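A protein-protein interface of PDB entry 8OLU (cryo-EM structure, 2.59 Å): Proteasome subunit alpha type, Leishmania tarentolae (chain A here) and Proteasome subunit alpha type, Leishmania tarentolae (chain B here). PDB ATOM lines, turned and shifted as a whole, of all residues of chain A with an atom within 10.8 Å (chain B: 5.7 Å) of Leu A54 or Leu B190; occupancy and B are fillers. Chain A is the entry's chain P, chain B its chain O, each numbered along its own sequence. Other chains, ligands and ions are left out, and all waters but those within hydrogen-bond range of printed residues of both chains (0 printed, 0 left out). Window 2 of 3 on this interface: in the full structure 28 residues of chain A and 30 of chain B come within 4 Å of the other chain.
The backbone NH of Arg B40 lies within hydrogen-bond range of the backbone carbonyl oxygen of Ile B166 (3.0 Å). O of Asp A56 is in hydrogen-bond range of OG of Ser A59, at 2.7 Å. The guanidinium group of Arg B40 is in salt-bridge range of the side-chain carboxylate of Asp B191, at 2.6 Å. OG of Ser A58 lies within hydrogen-bond range of OD1 of Asp A56, 2.8 Å away. The backbone NH (N) of Leu A54 sits close to the side-chain hydroxyl (OG) of Ser A52 (3.3 Å).
Of the 12 printed residues of chain A, 6 touch a printed residue of chain B. Printed residues of chain A that touch a printed residue of chain B: Ser A52, Thr A53, Leu A54, Val A55, Asp A56 and Ser A59. Hydrophobic or aromatic side chains of chain A within 4 Å of the printed part of chain B: Leu A54 and Val A55. Among the printed residues, 16 pairs touch across the chains.
N of Ala B167 sits at hydrogen-bond distance from O of Leu A54, 3.4 Å away. The backbone carbonyl oxygen (O) of Thr A53 lies within hydrogen-bond range of the side-chain amide nitrogen (NE2) of Gln B185, 3.1 Å away. NH2 of Arg B40 is in salt-bridge range of OD2 of Asp A56 (2.8 Å). The backbone NH (N) of Gly B164 sits at hydrogen-bond distance from the side-chain hydroxyl (OG) of Ser A59. The backbone NH (N) of Ile B166 lies within hydrogen-bond range of the backbone carbonyl oxygen (O) of Leu A54, at 2.7 Å. The backbone carbonyl oxygen (O) of Gly B164 is in hydrogen-bond range of the backbone NH (N) of Asp A56, at 3.1 Å.
Ser A52 touches Glu B182 (CB to OE1, 3.2 Å). Ile B166 touches Thr A53. CA of His B165 touches O of Leu A54 (3.5 Å). Met B178 touches Leu A54. Leu B181 touches Leu A54 (CB to CD1, 3.6 Å). Leu A54 touches Gln B185. Leu A54 touches Leu B190 (CD2 to CD1, 3.9 Å). Val A55 touches Gly B164. His B165 touches Val A55 (ND1 to CG2, 3.9 Å). N of Asp A56 touches CA of His B165 (3.7 Å).
Of the printed residues of chain B, Leu A54 touches His B165, Ile B166, Ala B167, Met B178, Leu B181, Gln B185 and Leu B190. Of chain A, only Leu A54 (3.9 Å) comes within 4 Å of Leu B190. No residue of chain A comes within 4 Å of Cys B41. Ile B166 touches just these residues of chain A: Thr A53 and Leu A54. Of the printed residues of chain A, Ala B167 touches Leu A54. Met B178 touches one residue of chain A. Gln B185 touches just these residues of chain A: Thr A53 (3.1 Å) and Leu A54 (3.5 Å). No residue of chain A comes within 4 Å of Thr B188. No residue of chain A comes within 4 Å of Ala B192. Leu B193 touches none of the printed residues of chain A. Of the printed residues of chain B, Asp A56 touches Arg B40 (2.8 Å), Gly B164 (3.1 Å) and His B165 (3.7 Å). Printed residues of chain A within 4 Å of Gly B164: Val A55, Asp A56 and Ser A59. Lys B42 touches none of the printed residues of chain A. The nearest printed residue of chain B that does not touch Ser A59 is His B165 (4.8 Å).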
ATOM      1  N   LYS A  49       8.379   2.057   8.452  1.00  0.00           N
ATOM      2  CA  LYS A  49       9.114   2.323   9.674  1.00  0.00           C
ATOM      3  C   LYS A  49      10.371   1.464   9.636  1.00  0.00           C
ATOM      4  O   LYS A  49      10.331   0.275   9.950  1.00  0.00           O
ATOM      5  CB  LYS A  49       8.260   2.106  10.925  1.00  0.00           C
ATOM      6  CG  LYS A  49       8.752   2.854  12.164  1.00  0.00           C
ATOM      7  CD  LYS A  49       7.910   2.606  13.402  1.00  0.00           C
ATOM      8  CE  LYS A  49       7.588   1.138  13.601  1.00  0.00           C
ATOM      9  NZ  LYS A  49       6.937   0.892  14.905  1.00  0.00           N
ATOM     10  N   ALA A  50      11.467   2.110   9.216  1.00  0.00           N
ATOM     11  CA  ALA A  50      12.794   1.520   9.142  1.00  0.00           C
ATOM     12  C   ALA A  50      13.352   1.258  10.548  1.00  0.00           C
ATOM     13  O   ALA A  50      13.351   2.156  11.396  1.00  0.00           O
ATOM     14  CB  ALA A  50      13.661   2.473   8.350  1.00  0.00           C
ATOM     15  N   PRO A  51      13.903   0.055  10.842  1.00  0.00           N
ATOM     16  CA  PRO A  51      14.385  -0.256  12.194  1.00  0.00           C
ATOM     17  C   PRO A  51      15.405   0.749  12.747  1.00  0.00           C
ATOM     18  O   PRO A  51      15.421   1.002  13.954  1.00  0.00           O
ATOM     19  CB  PRO A  51      15.017  -1.664  12.112  1.00  0.00           C
ATOM     20  CG  PRO A  51      15.061  -2.020  10.625  1.00  0.00           C
ATOM     21  CD  PRO A  51      14.131  -1.054   9.898  1.00  0.00           C
ATOM     22  N   SER A  52      16.254   1.294  11.853  1.00  0.00           N
ATOM     23  CA  SER A  52      17.322   2.218  12.203  1.00  0.00           C
ATOM     24  C   SER A  52      17.495   3.244  11.100  1.00  0.00           C
ATOM     25  O   SER A  52      17.002   3.058   9.993  1.00  0.00           O
ATOM     26  CB  SER A  52      18.628   1.500  12.420  1.00  0.00           C
ATOM     27  OG  SER A  52      19.132   0.933  11.220  1.00  0.00           O
ATOM     28  N   THR A  53      18.288   4.273  11.384  1.00  0.00           N
ATOM     29  CA  THR A  53      18.566   5.298  10.387  1.00  0.00           C
ATOM     30  C   THR A  53      19.595   4.817   9.361  1.00  0.00           C
ATOM     31  O   THR A  53      19.834   5.462   8.333  1.00  0.00           O
ATOM     32  CB  THR A  53      19.065   6.551  11.100  1.00  0.00           C
ATOM     33  OG1 THR A  53      18.962   6.202  12.486  1.00  0.00           O
ATOM     34  CG2 THR A  53      18.287   7.781  10.668  1.00  0.00           C
ATOM     35  N   LEU A  54      20.242   3.701   9.697  1.00  0.00           N
ATOM     36  CA  LEU A  54      21.305   3.172   8.871  1.00  0.00           C
ATOM     37  C   LEU A  54      20.778   2.287   7.750  1.00  0.00           C
ATOM     38  O   LEU A  54      21.510   1.933   6.842  1.00  0.00           O
ATOM     39  CB  LEU A  54      22.191   2.331   9.754  1.00  0.00           C
ATOM     40  CG  LEU A  54      22.901   3.071  10.868  1.00  0.00           C
ATOM     41  CD1 LEU A  54      23.548   2.010  11.741  1.00  0.00           C
ATOM     42  CD2 LEU A  54      23.926   4.045  10.312  1.00  0.00           C
ATOM     43  N   VAL A  55      19.509   1.955   7.805  1.00  0.00           N
ATOM     44  CA  VAL A  55      18.841   1.410   6.655  1.00  0.00           C
ATOM     45  C   VAL A  55      18.650   2.477   5.608  1.00  0.00           C
ATOM     46  O   VAL A  55      18.185   3.552   5.917  1.00  0.00           O
ATOM     47  CB  VAL A  55      17.482   0.835   7.050  1.00  0.00           C
ATOM     48  CG1 VAL A  55      16.734   0.376   5.826  1.00  0.00           C
ATOM     49  CG2 VAL A  55      17.632  -0.303   8.036  1.00  0.00           C
ATOM     50  N   ASP A  56      18.990   2.107   4.388  1.00  0.00           N
ATOM     51  CA  ASP A  56      18.781   2.881   3.188  1.00  0.00           C
ATOM     52  C   ASP A  56      17.304   2.777   2.889  1.00  0.00           C
ATOM     53  O   ASP A  56      16.864   1.754   2.385  1.00  0.00           O
ATOM     54  CB  ASP A  56      19.586   2.292   2.024  1.00  0.00           C
ATOM     55  CG  ASP A  56      19.471   3.061   0.720  1.00  0.00           C
ATOM     56  OD1 ASP A  56      18.434   3.784   0.534  1.00  0.00           O
ATOM     57  OD2 ASP A  56      20.424   2.975  -0.096  1.00  0.00           O
ATOM     58  N   ALA A  57      16.555   3.812   3.260  1.00  0.00           N
ATOM     59  CA  ALA A  57      15.111   3.797   3.147  1.00  0.00           C
ATOM     60  C   ALA A  57      14.686   3.763   1.678  1.00  0.00           C
ATOM     61  O   ALA A  57      13.622   3.270   1.358  1.00  0.00           O
ATOM     62  CB  ALA A  57      14.568   5.000   3.865  1.00  0.00           C
ATOM     63  N   SER A  58      15.525   4.211   0.756  1.00  0.00           N
ATOM     64  CA  SER A  58      15.171   4.034  -0.639  1.00  0.00           C
ATOM     65  C   SER A  58      14.904   2.556  -0.928  1.00  0.00           C
ATOM     66  O   SER A  58      14.050   2.222  -1.710  1.00  0.00           O
ATOM     67  CB  SER A  58      16.238   4.607  -1.562  1.00  0.00           C
ATOM     68  OG  SER A  58      17.160   3.593  -1.952  1.00  0.00           O
ATOM     69  N   SER A  59      15.661   1.653  -0.309  1.00  0.00           N
ATOM     70  CA  SER A  59      15.597   0.227  -0.606  1.00  0.00           C
ATOM     71  C   SER A  59      14.389  -0.468   0.029  1.00  0.00           C
ATOM     72  O   SER A  59      14.177  -1.644  -0.217  1.00  0.00           O
ATOM     73  CB  SER A  59      16.841  -0.457  -0.128  1.00  0.00           C
ATOM     74  OG  SER A  59      16.745  -0.703   1.305  1.00  0.00           O
ATOM     75  N   ILE A  60      13.667   0.184   0.932  1.00  0.00           N
ATOM     76  CA  ILE A  60      12.486  -0.452   1.475  1.00  0.00           C
ATOM     77  C   ILE A  60      11.295  -0.093   0.604  1.00  0.00           C
ATOM     78  O   ILE A  60      11.012   1.079   0.338  1.00  0.00           O
ATOM     79  CB  ILE A  60      12.216  -0.068   2.934  1.00  0.00           C
ATOM     80  CG1 ILE A  60      13.399  -0.397   3.833  1.00  0.00           C
ATOM     81  CG2 ILE A  60      10.959  -0.750   3.448  1.00  0.00           C
ATOM     82  CD1 ILE A  60      13.280   0.329   5.164  1.00  0.00           C
ATOM     83  N   ILE B  39      29.797  -1.195   5.726  1.00  0.00           N
ATOM     84  CA  ILE B  39      29.583   0.224   5.655  1.00  0.00           C
ATOM     85  C   ILE B  39      29.887   0.704   4.253  1.00  0.00           C
ATOM     86  O   ILE B  39      30.796   0.227   3.592  1.00  0.00           O
ATOM     87  CB  ILE B  39      30.441   0.952   6.700  1.00  0.00           C
ATOM     88  CG1 ILE B  39      30.246   2.458   6.669  1.00  0.00           C
ATOM     89  CG2 ILE B  39      31.904   0.663   6.484  1.00  0.00           C
ATOM     90  CD1 ILE B  39      30.579   3.134   8.016  1.00  0.00           C
ATOM     91  N   ARG B  40      29.097   1.637   3.782  1.00  0.00           N
ATOM     92  CA  ARG B  40      29.411   2.169   2.488  1.00  0.00           C
ATOM     93  C   ARG B  40      29.792   3.619   2.662  1.00  0.00           C
ATOM     94  O   ARG B  40      29.257   4.331   3.498  1.00  0.00           O
ATOM     95  CB  ARG B  40      28.295   1.949   1.455  1.00  0.00           C
ATOM     96  CG  ARG B  40      26.950   2.502   1.856  1.00  0.00           C
ATOM     97  CD  ARG B  40      25.899   2.378   0.784  1.00  0.00           C
ATOM     98  NE  ARG B  40      25.106   3.580   0.957  1.00  0.00           N
ATOM     99  CZ  ARG B  40      23.891   3.773   0.504  1.00  0.00           C
ATOM    100  NH1 ARG B  40      23.400   4.998   0.444  1.00  0.00           N
ATOM    101  NH2 ARG B  40      23.178   2.734   0.136  1.00  0.00           N
ATOM    102  N   CYS B  41      30.746   4.000   1.818  1.00  0.00           N
ATOM    103  CA  CYS B  41      31.224   5.367   1.695  1.00  0.00           C
ATOM    104  C   CYS B  41      30.900   5.848   0.288  1.00  0.00           C
ATOM    105  O   CYS B  41      30.107   5.201  -0.392  1.00  0.00           O
ATOM    106  CB  CYS B  41      32.703   5.363   2.040  1.00  0.00           C
ATOM    107  SG  CYS B  41      33.706   4.482   0.815  1.00  0.00           S
ATOM    108  N   LYS B  42      31.445   6.991  -0.140  1.00  0.00           N
ATOM    109  CA  LYS B  42      30.972   7.588  -1.390  1.00  0.00           C
ATOM    110  C   LYS B  42      31.300   6.673  -2.572  1.00  0.00           C
ATOM    111  O   LYS B  42      30.464   6.503  -3.460  1.00  0.00           O
ATOM    112  CB  LYS B  42      31.507   9.013  -1.592  1.00  0.00           C
ATOM    113  CG  LYS B  42      33.012   9.099  -1.786  1.00  0.00           C
ATOM    114  CD  LYS B  42      33.613  10.485  -1.682  1.00  0.00           C
ATOM    115  CE  LYS B  42      35.130  10.408  -1.670  1.00  0.00           C
ATOM    116  NZ  LYS B  42      35.734  11.708  -1.310  1.00  0.00           N
ATOM    117  N   GLY B 164      18.314  -3.003   1.983  1.00  0.00           N
ATOM    118  CA  GLY B 164      19.533  -2.254   1.701  1.00  0.00           C
ATOM    119  C   GLY B 164      19.922  -1.375   2.876  1.00  0.00           C
ATOM    120  O   GLY B 164      19.063  -0.891   3.583  1.00  0.00           O
ATOM    121  N   HIS B 165      21.214  -1.139   3.050  1.00  0.00           N
ATOM    122  CA  HIS B 165      21.717  -0.417   4.199  1.00  0.00           C
ATOM    123  C   HIS B 165      22.829   0.534   3.814  1.00  0.00           C
ATOM    124  O   HIS B 165      23.467   0.359   2.787  1.00  0.00           O
ATOM    125  CB  HIS B 165      22.303  -1.397   5.157  1.00  0.00           C
ATOM    126  CG  HIS B 165      21.357  -2.373   5.734  1.00  0.00           C
ATOM    127  ND1 HIS B 165      20.849  -2.251   6.996  1.00  0.00           N
ATOM    128  CD2 HIS B 165      21.060  -3.626   5.284  1.00  0.00           C
ATOM    129  CE1 HIS B 165      20.174  -3.372   7.272  1.00  0.00           C
ATOM    130  NE2 HIS B 165      20.297  -4.250   6.221  1.00  0.00           N
ATOM    131  N   ILE B 166      23.034   1.507   4.684  1.00  0.00           N
ATOM    132  CA  ILE B 166      24.161   2.411   4.648  1.00  0.00           C
ATOM    133  C   ILE B 166      25.273   1.840   5.510  1.00  0.00           C
ATOM    134  O   ILE B 166      26.458   1.972   5.252  1.00  0.00           O
ATOM    135  CB  ILE B 166      23.711   3.755   5.233  1.00  0.00           C
ATOM    136  CG1 ILE B 166      22.532   4.330   4.455  1.00  0.00           C
ATOM    137  CG2 ILE B 166      24.837   4.759   5.304  1.00  0.00           C
ATOM    138  CD1 ILE B 166      21.919   5.489   5.185  1.00  0.00           C
ATOM    139  N   ALA B 167      24.874   1.288   6.618  1.00  0.00           N
ATOM    140  CA  ALA B 167      25.802   0.513   7.391  1.00  0.00           C
ATOM    141  C   ALA B 167      24.978  -0.460   8.180  1.00  0.00           C
ATOM    142  O   ALA B 167      23.786  -0.270   8.346  1.00  0.00           O
ATOM    143  CB  ALA B 167      26.584   1.373   8.328  1.00  0.00           C
ATOM    144  N   CYS B 168      25.615  -1.526   8.602  1.00  0.00           N
ATOM    145  CA  CYS B 168      24.843  -2.594   9.171  1.00  0.00           C
ATOM    146  C   CYS B 168      25.789  -3.479   9.904  1.00  0.00           C
ATOM    147  O   CYS B 168      26.930  -3.607   9.516  1.00  0.00           O
ATOM    148  CB  CYS B 168      24.052  -3.340   8.118  1.00  0.00           C
ATOM    149  SG  CYS B 168      24.998  -4.618   7.280  1.00  0.00           S
ATOM    150  N   MET B 178      25.437  -1.190  16.288  1.00  0.00           N
ATOM    151  CA  MET B 178      24.498  -0.373  15.519  1.00  0.00           C
ATOM    152  C   MET B 178      24.375   0.995  16.176  1.00  0.00           C
ATOM    153  O   MET B 178      24.530   2.006  15.496  1.00  0.00           O
ATOM    154  CB  MET B 178      23.091  -0.988  15.480  1.00  0.00           C
ATOM    155  CG  MET B 178      22.887  -2.025  14.399  1.00  0.00           C
ATOM    156  SD  MET B 178      23.482  -1.470  12.783  1.00  0.00           S
ATOM    157  CE  MET B 178      22.156  -2.084  11.734  1.00  0.00           C
ATOM    158  N   LEU B 181      27.036   3.228  15.378  1.00  0.00           N
ATOM    159  CA  LEU B 181      27.042   3.770  14.029  1.00  0.00           C
ATOM    160  C   LEU B 181      25.921   4.788  13.877  1.00  0.00           C
ATOM    161  O   LEU B 181      26.049   5.708  13.088  1.00  0.00           O
ATOM    162  CB  LEU B 181      26.807   2.634  13.031  1.00  0.00           C
ATOM    163  CG  LEU B 181      27.950   1.661  12.884  1.00  0.00           C
ATOM    164  CD1 LEU B 181      27.505   0.413  12.180  1.00  0.00           C
ATOM    165  CD2 LEU B 181      29.079   2.299  12.118  1.00  0.00           C
ATOM    166  N   GLU B 182      24.792   4.576  14.556  1.00  0.00           N
ATOM    167  CA  GLU B 182      23.715   5.546  14.535  1.00  0.00           C
ATOM    168  C   GLU B 182      24.334   6.819  15.080  1.00  0.00           C
ATOM    169  O   GLU B 182      24.277   7.853  14.432  1.00  0.00           O
ATOM    170  CB  GLU B 182      22.492   5.089  15.356  1.00  0.00           C
ATOM    171  CG  GLU B 182      21.629   3.995  14.696  1.00  0.00           C
ATOM    172  CD  GLU B 182      20.971   2.924  15.588  1.00  0.00           C
ATOM    173  OE1 GLU B 182      20.499   1.888  15.024  1.00  0.00           O
ATOM    174  OE2 GLU B 182      20.914   3.100  16.849  1.00  0.00           O
ATOM    175  N   ARG B 184      27.382   7.828  15.278  1.00  0.00           N
ATOM    176  CA  ARG B 184      28.362   8.445  14.408  1.00  0.00           C
ATOM    177  C   ARG B 184      27.717   8.933  13.113  1.00  0.00           C
ATOM    178  O   ARG B 184      28.387   9.578  12.311  1.00  0.00           O
ATOM    179  CB  ARG B 184      29.501   7.471  14.084  1.00  0.00           C
ATOM    180  CG  ARG B 184      30.822   8.160  13.756  1.00  0.00           C
ATOM    181  CD  ARG B 184      31.546   8.680  14.995  1.00  0.00           C
ATOM    182  NE  ARG B 184      32.590   7.784  15.487  1.00  0.00           N
ATOM    183  CZ  ARG B 184      33.736   7.530  14.849  1.00  0.00           C
ATOM    184  NH1 ARG B 184      34.622   6.695  15.375  1.00  0.00           N
ATOM    185  NH2 ARG B 184      33.990   8.110  13.683  1.00  0.00           N
ATOM    186  N   GLN B 185      26.437   8.611  12.893  1.00  0.00           N
ATOM    187  CA  GLN B 185      25.692   9.069  11.727  1.00  0.00           C
ATOM    188  C   GLN B 185      24.961  10.380  12.024  1.00  0.00           C
ATOM    189  O   GLN B 185      24.420  11.006  11.114  1.00  0.00           O
ATOM    190  CB  GLN B 185      24.644   8.020  11.346  1.00  0.00           C
ATOM    191  CG  GLN B 185      24.087   8.121   9.938  1.00  0.00           C
ATOM    192  CD  GLN B 185      22.773   7.402   9.801  1.00  0.00           C
ATOM    193  OE1 GLN B 185      22.165   7.037  10.808  1.00  0.00           O
ATOM    194  NE2 GLN B 185      22.339   7.194   8.556  1.00  0.00           N
ATOM    195  N   THR B 188      28.477  12.817  11.220  1.00  0.00           N
ATOM    196  CA  THR B 188      28.882  12.899   9.824  1.00  0.00           C
ATOM    197  C   THR B 188      27.756  12.382   8.924  1.00  0.00           C
ATOM    198  O   THR B 188      26.770  11.817   9.388  1.00  0.00           O
ATOM    199  CB  THR B 188      30.238  12.188   9.588  1.00  0.00           C
ATOM    200  OG1 THR B 188      30.243  10.844  10.084  1.00  0.00           O
ATOM    201  CG2 THR B 188      31.414  12.918  10.212  1.00  0.00           C
ATOM    202  N   GLU B 189      27.914  12.618   7.623  1.00  0.00           N
ATOM    203  CA  GLU B 189      27.075  11.998   6.617  1.00  0.00           C
ATOM    204  C   GLU B 189      27.878  10.840   6.038  1.00  0.00           C
ATOM    205  O   GLU B 189      28.975  11.038   5.526  1.00  0.00           O
ATOM    206  CB  GLU B 189      26.668  13.038   5.561  1.00  0.00           C
ATOM    207  CG  GLU B 189      25.209  12.934   5.111  1.00  0.00           C
ATOM    208  CD  GLU B 189      24.887  11.967   3.975  1.00  0.00           C
ATOM    209  OE1 GLU B 189      25.826  11.337   3.437  1.00  0.00           O
ATOM    210  OE2 GLU B 189      23.692  11.860   3.611  1.00  0.00           O
ATOM    211  N   LEU B 190      27.336   9.631   6.117  1.00  0.00           N
ATOM    212  CA  LEU B 190      28.151   8.454   5.902  1.00  0.00           C
ATOM    213  C   LEU B 190      28.425   8.187   4.424  1.00  0.00           C
ATOM    214  O   LEU B 190      29.382   7.480   4.111  1.00  0.00           O
ATOM    215  CB  LEU B 190      27.474   7.245   6.555  1.00  0.00           C
ATOM    216  CG  LEU B 190      27.534   7.174   8.075  1.00  0.00           C
ATOM    217  CD1 LEU B 190      26.926   5.871   8.567  1.00  0.00           C
ATOM    218  CD2 LEU B 190      28.954   7.287   8.601  1.00  0.00           C
ATOM    219  N   ASP B 191      27.598   8.711   3.515  1.00  0.00           N
ATOM    220  CA  ASP B 191      27.783   8.458   2.087  1.00  0.00           C
ATOM    221  C   ASP B 191      28.668   9.527   1.434  1.00  0.00           C
ATOM    222  O   ASP B 191      28.820   9.534   0.212  1.00  0.00           O
ATOM    223  CB  ASP B 191      26.429   8.360   1.362  1.00  0.00           C
ATOM    224  CG  ASP B 191      25.616   7.113   1.687  1.00  0.00           C
ATOM    225  OD1 ASP B 191      26.056   6.004   1.293  1.00  0.00           O
ATOM    226  OD2 ASP B 191      24.554   7.262   2.340  1.00  0.00           O
ATOM    227  N   ALA B 192      29.193  10.458   2.246  1.00  0.00           N
ATOM    228  CA  ALA B 192      30.125  11.477   1.798  1.00  0.00           C
ATOM    229  C   ALA B 192      31.529  11.220   2.347  1.00  0.00           C
ATOM    230  O   ALA B 192      32.425  12.031   2.133  1.00  0.00           O
ATOM    231  CB  ALA B 192      29.623  12.824   2.235  1.00  0.00           C
ATOM    232  N   LEU B 193      31.713  10.087   3.034  1.00  0.00           N
ATOM    233  CA  LEU B 193      32.981   9.709   3.629  1.00  0.00           C
ATOM    234  C   LEU B 193      33.907   9.111   2.594  1.00  0.00           C
ATOM    235  O   LEU B 193      33.512   8.838   1.470  1.00  0.00           O
ATOM    236  CB  LEU B 193      32.716   8.652   4.698  1.00  0.00           C
ATOM    237  CG  LEU B 193      32.703   9.161   6.135  1.00  0.00           C
ATOM    238  CD1 LEU B 193      32.120  10.576   6.237  1.00  0.00           C
ATOM    239  CD2 LEU B 193      31.972   8.169   7.019  1.00  0.00           C
ATOM    240  N   ILE B 201      35.390   4.078  10.987  1.00  0.00           N
ATOM    241  CA  ILE B 201      34.107   3.929  11.656  1.00  0.00           C
ATOM    242  C   ILE B 201      33.708   2.466  11.840  1.00  0.00           C
ATOM    243  O   ILE B 201      33.262   2.082  12.908  1.00  0.00           O
ATOM    244  CB  ILE B 201      33.026   4.678  10.885  1.00  0.00           C
ATOM    245  CG1 ILE B 201      33.284   6.170  10.944  1.00  0.00           C
ATOM    246  CG2 ILE B 201      31.680   4.349  11.450  1.00  0.00           C
ATOM    247  CD1 ILE B 201      32.302   6.982  10.133  1.00  0.00           C
